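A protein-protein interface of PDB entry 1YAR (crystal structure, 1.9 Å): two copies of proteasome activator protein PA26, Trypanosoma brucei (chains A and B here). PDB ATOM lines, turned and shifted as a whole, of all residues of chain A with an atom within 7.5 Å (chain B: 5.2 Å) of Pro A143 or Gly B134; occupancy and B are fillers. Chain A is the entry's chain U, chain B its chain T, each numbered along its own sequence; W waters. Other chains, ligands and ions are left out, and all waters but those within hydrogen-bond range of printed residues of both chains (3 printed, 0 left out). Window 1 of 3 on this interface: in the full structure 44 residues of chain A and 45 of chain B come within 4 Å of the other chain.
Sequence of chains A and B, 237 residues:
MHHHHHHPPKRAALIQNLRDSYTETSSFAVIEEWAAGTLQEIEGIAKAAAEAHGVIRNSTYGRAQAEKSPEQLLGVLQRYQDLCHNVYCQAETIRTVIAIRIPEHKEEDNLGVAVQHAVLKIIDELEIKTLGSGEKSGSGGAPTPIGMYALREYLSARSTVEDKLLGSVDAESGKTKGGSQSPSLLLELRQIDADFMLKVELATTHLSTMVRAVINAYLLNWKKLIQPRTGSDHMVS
O of Ala A142 lies within hydrogen-bond range of N of Glu B135 (2.9 Å). The backbone carbonyl oxygen of Thr A144 sits at hydrogen-bond distance from the backbone NH of Glu B135 (3.1 Å). The backbone carbonyl oxygen (O) of Lys B136 is in hydrogen-bond range of the backbone NH (N) of Ala A142, at 2.8 Å.
OG of Ser B133 sits at hydrogen-bond distance from O of Glu B127, 2.7 Å away. The backbone carbonyl oxygen (O) of Ser B133 is in hydrogen-bond range of the side-chain hydroxyl (OH) of Tyr B149, at 2.7 Å. O of Thr A130 sits at hydrogen-bond distance from OG1 of Thr A144, at 3.1 Å. The side-chain hydroxyl (OG1) of Thr A144 lies within hydrogen-bond range of the backbone carbonyl oxygen (O) of Ile A146 (3.1 Å).
Ala A142 touches Gly B134. O of Pro A143 touches CD1 of Ile B128 (3.7 Å). O of Pro A143 touches CA of Gly B134, 3.3 Å away. Thr A144 touches Gly B134. Ser B133 touches Pro A145. Pro A145 touches Glu B135 (O to CB, 3.6 Å). OH of Tyr B149 touches CB of Pro A145, 3.5 Å away. Glu B135 touches Ile A146 (OE1 to CA, 3.6 Å). CE2 of Tyr B149 touches CG of Lys A199, 3.7 Å away. OH of Tyr B149 touches CD1 of Leu A202, 3.7 Å away.
Pro A143 touches just these residues of chain B: Ile B128 and Gly B134. Of chain A, only Ala A142, Pro A143 and Thr A144 come within 4 Å of Gly B134. Of the printed residues of chain A, Ser B133 touches Pro A145. Of the printed residues of chain B, Leu A202 touches Tyr B149. Of the printed residues of chain B, Gly A141 touches Lys B136. Of the printed residues of chain B, Pro A145 touches Ser B133, Glu B135 and Tyr B149. His A206 touches none of the printed residues of chain B.
Of the 8 printed residues of chain B, 6 touch a printed residue of chain A. Hydrophobic or aromatic side chains of chain B that line the printed part of chain A: Ile B128 and Tyr B149. Among the printed residues, 14 pairs touch across the chains. Among the printed residues, no Asp or Glu carboxylate lies within 4 Å of a Lys or Arg side-chain nitrogen of the other chain.
Positions printed for both chains: 128 and 132. Of the 14 pairs that touch across the chains among the printed residues, none has its exchanged pair printed and touching as well.
Water W3 lies within hydrogen-bond range of OE1 of Glu B135 (2.5 Å), NZ of Lys A199 (3.1 Å) and O of Pro A145 (3.2 Å). Water W1 bridges the backbone carbonyl oxygen of Pro A143 and the side-chain hydroxyl of Ser B133. Water W2 bridges OE1 of Glu B127 (2.9 Å) and ND1 of His A206 (3.3 Å).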
ATOM      1  N   GLU A 125       8.633  -2.227  23.499  1.00  0.00           N
ATOM      2  CA  GLU A 125       8.978  -3.643  23.481  1.00  0.00           C
ATOM      3  C   GLU A 125       9.440  -4.092  24.866  1.00  0.00           C
ATOM      4  O   GLU A 125       8.998  -5.120  25.356  1.00  0.00           O
ATOM      5  CB  GLU A 125      10.073  -3.947  22.473  1.00  0.00           C
ATOM      6  CG  GLU A 125      10.260  -5.443  22.250  1.00  0.00           C
ATOM      7  CD  GLU A 125      11.442  -5.781  21.350  1.00  0.00           C
ATOM      8  OE1 GLU A 125      11.994  -4.880  20.667  1.00  0.00           O
ATOM      9  OE2 GLU A 125      11.838  -6.967  21.336  1.00  0.00           O
ATOM     10  N   ILE A 128       6.182  -3.935  27.307  1.00  0.00           N
ATOM     11  CA  ILE A 128       5.058  -4.790  26.957  1.00  0.00           C
ATOM     12  C   ILE A 128       5.505  -6.233  26.751  1.00  0.00           C
ATOM     13  O   ILE A 128       4.901  -7.146  27.304  1.00  0.00           O
ATOM     14  CB  ILE A 128       4.319  -4.215  25.689  1.00  0.00           C
ATOM     15  CG1 ILE A 128       3.775  -2.803  25.967  1.00  0.00           C
ATOM     16  CG2 ILE A 128       3.238  -5.212  25.131  1.00  0.00           C
ATOM     17  CD1 ILE A 128       2.875  -2.696  27.210  1.00  0.00           C
ATOM     18  N   LYS A 129       6.553  -6.445  25.961  1.00  0.00           N
ATOM     19  CA  LYS A 129       6.978  -7.794  25.646  1.00  0.00           C
ATOM     20  C   LYS A 129       7.973  -8.315  26.695  1.00  0.00           C
ATOM     21  O   LYS A 129       7.753  -9.377  27.273  1.00  0.00           O
ATOM     22  CB  LYS A 129       7.575  -7.881  24.241  1.00  0.00           C
ATOM     23  CG  LYS A 129       6.578  -7.480  23.116  1.00  0.00           C
ATOM     24  CD  LYS A 129       7.103  -7.963  21.774  1.00  0.00           C
ATOM     25  CE  LYS A 129       6.763  -7.018  20.628  1.00  0.00           C
ATOM     26  NZ  LYS A 129       7.600  -7.346  19.425  1.00  0.00           N
ATOM     27  N   THR A 130       9.036  -7.572  26.966  1.00  0.00           N
ATOM     28  CA  THR A 130      10.114  -8.126  27.818  1.00  0.00           C
ATOM     29  C   THR A 130       9.643  -8.284  29.254  1.00  0.00           C
ATOM     30  O   THR A 130       9.877  -9.338  29.876  1.00  0.00           O
ATOM     31  CB  THR A 130      11.374  -7.258  27.762  1.00  0.00           C
ATOM     32  OG1 THR A 130      11.741  -7.062  26.394  1.00  0.00           O
ATOM     33  CG2 THR A 130      12.580  -7.995  28.352  1.00  0.00           C
ATOM     34  N   GLY A 132       6.423  -8.090  30.150  1.00  0.00           N
ATOM     35  CA  GLY A 132       5.096  -8.715  30.233  1.00  0.00           C
ATOM     36  C   GLY A 132       4.149  -7.939  31.153  1.00  0.00           C
ATOM     37  O   GLY A 132       3.427  -8.524  31.950  1.00  0.00           O
ATOM     38  N   SER A 137      -1.601 -10.603  26.736  1.00  0.00           N
ATOM     39  CA  SER A 137      -0.652 -10.635  25.631  1.00  0.00           C
ATOM     40  C   SER A 137      -1.347 -10.459  24.290  1.00  0.00           C
ATOM     41  O   SER A 137      -2.486 -10.896  24.114  1.00  0.00           O
ATOM     42  CB  SER A 137       0.075 -11.984  25.636  1.00  0.00           C
ATOM     43  OG  SER A 137       1.082 -11.989  26.625  1.00  0.00           O
ATOM     44  N   GLY A 140       0.853 -11.668  19.042  1.00  0.00           N
ATOM     45  CA  GLY A 140       2.265 -12.044  18.932  1.00  0.00           C
ATOM     46  C   GLY A 140       2.797 -12.950  20.047  1.00  0.00           C
ATOM     47  O   GLY A 140       3.982 -13.326  20.040  1.00  0.00           O
ATOM     48  N   GLY A 141       1.939 -13.286  21.006  1.00  0.00           N
ATOM     49  CA  GLY A 141       2.292 -14.171  22.113  1.00  0.00           C
ATOM     50  C   GLY A 141       3.017 -13.473  23.266  1.00  0.00           C
ATOM     51  O   GLY A 141       2.992 -12.240  23.400  1.00  0.00           O
ATOM     52  N   ALA A 142       3.667 -14.271  24.101  1.00  0.00           N
ATOM     53  CA  ALA A 142       4.450 -13.723  25.209  1.00  0.00           C
ATOM     54  C   ALA A 142       5.867 -14.300  25.085  1.00  0.00           C
ATOM     55  O   ALA A 142       6.141 -15.406  25.562  1.00  0.00           O
ATOM     56  CB  ALA A 142       3.795 -14.084  26.535  1.00  0.00           C
ATOM     57  N   PRO A 143       6.751 -13.579  24.397  1.00  0.00           N
ATOM     58  CA  PRO A 143       8.081 -14.113  24.106  1.00  0.00           C
ATOM     59  C   PRO A 143       9.006 -14.159  25.319  1.00  0.00           C
ATOM     60  O   PRO A 143      10.002 -14.881  25.269  1.00  0.00           O
ATOM     61  CB  PRO A 143       8.636 -13.163  23.034  1.00  0.00           C
ATOM     62  CG  PRO A 143       7.918 -11.850  23.282  1.00  0.00           C
ATOM     63  CD  PRO A 143       6.561 -12.222  23.842  1.00  0.00           C
ATOM     64  N   THR A 144       8.702 -13.417  26.387  1.00  0.00           N
ATOM     65  CA  THR A 144       9.565 -13.489  27.582  1.00  0.00           C
ATOM     66  C   THR A 144       9.308 -14.817  28.322  1.00  0.00           C
ATOM     67  O   THR A 144       8.156 -15.278  28.351  1.00  0.00           O
ATOM     68  CB  THR A 144       9.346 -12.271  28.497  1.00  0.00           C
ATOM     69  OG1 THR A 144      10.201 -12.390  29.645  1.00  0.00           O
ATOM     70  CG2 THR A 144       7.915 -12.250  29.076  1.00  0.00           C
ATOM     71  N   PRO A 145      10.345 -15.481  28.857  1.00  0.00           N
ATOM     72  CA  PRO A 145      10.120 -16.721  29.612  1.00  0.00           C
ATOM     73  C   PRO A 145       9.175 -16.573  30.803  1.00  0.00           C
ATOM     74  O   PRO A 145       8.487 -17.520  31.162  1.00  0.00           O
ATOM     75  CB  PRO A 145      11.527 -17.122  30.062  1.00  0.00           C
ATOM     76  CG  PRO A 145      12.412 -16.553  28.952  1.00  0.00           C
ATOM     77  CD  PRO A 145      11.779 -15.205  28.684  1.00  0.00           C
ATOM     78  N   ILE A 146       9.134 -15.394  31.398  1.00  0.00           N
ATOM     79  CA  ILE A 146       8.239 -15.144  32.519  1.00  0.00           C
ATOM     80  C   ILE A 146       8.001 -13.655  32.604  1.00  0.00           C
ATOM     81  O   ILE A 146       8.917 -12.859  32.393  1.00  0.00           O
ATOM     82  CB  ILE A 146       8.794 -15.748  33.866  1.00  0.00           C
ATOM     83  CG1 ILE A 146       7.752 -15.656  34.973  1.00  0.00           C
ATOM     84  CG2 ILE A 146      10.087 -15.031  34.357  1.00  0.00           C
ATOM     85  CD1 ILE A 146       8.156 -16.423  36.246  1.00  0.00           C
ATOM     86  N   LYS A 199      13.076 -20.104  34.369  1.00  0.00           N
ATOM     87  CA  LYS A 199      12.460 -18.991  33.640  1.00  0.00           C
ATOM     88  C   LYS A 199      13.008 -17.665  34.128  1.00  0.00           C
ATOM     89  O   LYS A 199      13.249 -16.751  33.331  1.00  0.00           O
ATOM     90  CB  LYS A 199      10.941 -19.026  33.781  1.00  0.00           C
ATOM     91  CG  LYS A 199      10.284 -20.159  32.934  1.00  0.00           C
ATOM     92  CD  LYS A 199       8.789 -20.303  33.287  1.00  0.00           C
ATOM     93  CE  LYS A 199       8.026 -21.011  32.148  1.00  0.00           C
ATOM     94  NZ  LYS A 199       6.665 -21.339  32.647  1.00  0.00           N
ATOM     95  N   LEU A 202      16.464 -17.333  32.497  1.00  0.00           N
ATOM     96  CA  LEU A 202      16.352 -16.946  31.088  1.00  0.00           C
ATOM     97  C   LEU A 202      15.857 -15.509  30.915  1.00  0.00           C
ATOM     98  O   LEU A 202      16.407 -14.757  30.120  1.00  0.00           O
ATOM     99  CB  LEU A 202      15.439 -17.920  30.331  1.00  0.00           C
ATOM    100  CG  LEU A 202      15.786 -19.421  30.362  1.00  0.00           C
ATOM    101  CD1 LEU A 202      14.670 -20.246  29.661  1.00  0.00           C
ATOM    102  CD2 LEU A 202      17.141 -19.694  29.721  1.00  0.00           C
ATOM    103  N   HIS A 206      17.634 -12.238  29.124  1.00  0.00           N
ATOM    104  CA  HIS A 206      16.909 -11.582  28.017  1.00  0.00           C
ATOM    105  C   HIS A 206      16.705 -10.084  28.339  1.00  0.00           C
ATOM    106  O   HIS A 206      16.888  -9.206  27.482  1.00  0.00           O
ATOM    107  CB  HIS A 206      15.566 -12.305  27.856  1.00  0.00           C
ATOM    108  CG  HIS A 206      14.793 -11.924  26.631  1.00  0.00           C
ATOM    109  ND1 HIS A 206      15.300 -12.057  25.354  1.00  0.00           N
ATOM    110  CD2 HIS A 206      13.521 -11.480  26.488  1.00  0.00           C
ATOM    111  CE1 HIS A 206      14.382 -11.680  24.477  1.00  0.00           C
ATOM    112  NE2 HIS A 206      13.297 -11.319  25.142  1.00  0.00           N
ATOM    113  N   GLU B 127      15.686 -18.439  19.335  1.00  0.00           N
ATOM    114  CA  GLU B 127      15.306 -18.325  20.756  1.00  0.00           C
ATOM    115  C   GLU B 127      13.820 -18.497  20.968  1.00  0.00           C
ATOM    116  O   GLU B 127      13.413 -19.222  21.875  1.00  0.00           O
ATOM    117  CB  GLU B 127      15.768 -16.982  21.357  1.00  0.00           C
ATOM    118  CG  GLU B 127      17.270 -16.837  21.451  1.00  0.00           C
ATOM    119  CD  GLU B 127      17.731 -15.671  22.334  1.00  0.00           C
ATOM    120  OE1 GLU B 127      17.173 -15.468  23.418  1.00  0.00           O
ATOM    121  OE2 GLU B 127      18.678 -14.960  21.962  1.00  0.00           O
ATOM    122  N   ILE B 128      13.002 -17.859  20.132  1.00  0.00           N
ATOM    123  CA  ILE B 128      11.554 -17.833  20.376  1.00  0.00           C
ATOM    124  C   ILE B 128      10.878 -19.067  19.778  1.00  0.00           C
ATOM    125  O   ILE B 128      10.060 -19.711  20.425  1.00  0.00           O
ATOM    126  CB  ILE B 128      10.919 -16.518  19.817  1.00  0.00           C
ATOM    127  CG1 ILE B 128      11.565 -15.260  20.457  1.00  0.00           C
ATOM    128  CG2 ILE B 128       9.362 -16.526  19.911  1.00  0.00           C
ATOM    129  CD1 ILE B 128      11.642 -15.258  21.960  1.00  0.00           C
ATOM    130  N   GLY B 132      11.491 -22.519  21.765  1.00  0.00           N
ATOM    131  CA  GLY B 132      10.190 -22.382  22.410  1.00  0.00           C
ATOM    132  C   GLY B 132      10.248 -21.801  23.820  1.00  0.00           C
ATOM    133  O   GLY B 132       9.644 -22.337  24.758  1.00  0.00           O
ATOM    134  N   SER B 133      10.962 -20.696  23.967  1.00  0.00           N
ATOM    135  CA  SER B 133      11.335 -20.208  25.293  1.00  0.00           C
ATOM    136  C   SER B 133      10.297 -19.257  25.887  1.00  0.00           C
ATOM    137  O   SER B 133      10.295 -19.007  27.092  1.00  0.00           O
ATOM    138  CB  SER B 133      12.699 -19.521  25.207  1.00  0.00           C
ATOM    139  OG  SER B 133      12.604 -18.390  24.367  1.00  0.00           O
ATOM    140  N   GLY B 134       9.405 -18.741  25.044  1.00  0.00           N
ATOM    141  CA  GLY B 134       8.387 -17.784  25.489  1.00  0.00           C
ATOM    142  C   GLY B 134       7.322 -18.464  26.328  1.00  0.00           C
ATOM    143  O   GLY B 134       7.083 -19.671  26.194  1.00  0.00           O
ATOM    144  N   GLU B 135       6.666 -17.705  27.200  1.00  0.00           N
ATOM    145  CA  GLU B 135       5.616 -18.318  27.990  1.00  0.00           C
ATOM    146  C   GLU B 135       4.325 -18.565  27.195  1.00  0.00           C
ATOM    147  O   GLU B 135       3.591 -19.485  27.523  1.00  0.00           O
ATOM    148  CB  GLU B 135       5.384 -17.622  29.337  1.00  0.00           C
ATOM    149  CG  GLU B 135       5.158 -16.118  29.321  1.00  0.00           C
ATOM    150  CD  GLU B 135       4.609 -15.624  30.655  1.00  0.00           C
ATOM    151  OE1 GLU B 135       4.955 -16.244  31.696  1.00  0.00           O
ATOM    152  OE2 GLU B 135       3.815 -14.636  30.662  1.00  0.00           O
ATOM    153  N   LYS B 136       4.084 -17.773  26.146  1.00  0.00           N
ATOM    154  CA  LYS B 136       2.975 -18.030  25.196  1.00  0.00           C
ATOM    155  C   LYS B 136       3.443 -17.883  23.751  1.00  0.00           C
ATOM    156  O   LYS B 136       4.076 -16.896  23.382  1.00  0.00           O
ATOM    157  CB  LYS B 136       1.798 -17.067  25.429  1.00  0.00           C
ATOM    158  CG  LYS B 136       1.017 -17.318  26.699  1.00  0.00           C
ATOM    159  CD  LYS B 136      -0.245 -16.418  26.798  1.00  0.00           C
ATOM    160  CE  LYS B 136      -1.016 -16.712  28.098  1.00  0.00           C
ATOM    161  NZ  LYS B 136      -2.484 -16.356  28.036  1.00  0.00           N
ATOM    162  N   TYR B 149      10.282 -26.160  27.777  1.00  0.00           N
ATOM    163  CA  TYR B 149       9.571 -26.677  28.958  1.00  0.00           C
ATOM    164  C   TYR B 149       8.955 -28.049  28.653  1.00  0.00           C
ATOM    165  O   TYR B 149       7.856 -28.357  29.092  1.00  0.00           O
ATOM    166  CB  TYR B 149       8.535 -25.639  29.439  1.00  0.00           C
ATOM    167  CG  TYR B 149       9.156 -24.242  29.425  1.00  0.00           C
ATOM    168  CD1 TYR B 149       8.728 -23.271  28.509  1.00  0.00           C
ATOM    169  CD2 TYR B 149      10.248 -23.934  30.255  1.00  0.00           C
ATOM    170  CE1 TYR B 149       9.346 -21.991  28.455  1.00  0.00           C
ATOM    171  CE2 TYR B 149      10.858 -22.670  30.225  1.00  0.00           C
ATOM    172  CZ  TYR B 149      10.402 -21.710  29.317  1.00  0.00           C
ATOM    173  OH  TYR B 149      11.013 -20.475  29.257  1.00  0.00           O
HETATM  174  O   HOH W   1      12.411 -15.732  25.246  1.00  0.00           O
HETATM  175  O   HOH W   2      14.602 -14.215  22.963  1.00  0.00           O
HETATM  176  O   HOH W   3       5.782 -18.375  32.599  1.00  0.00           O
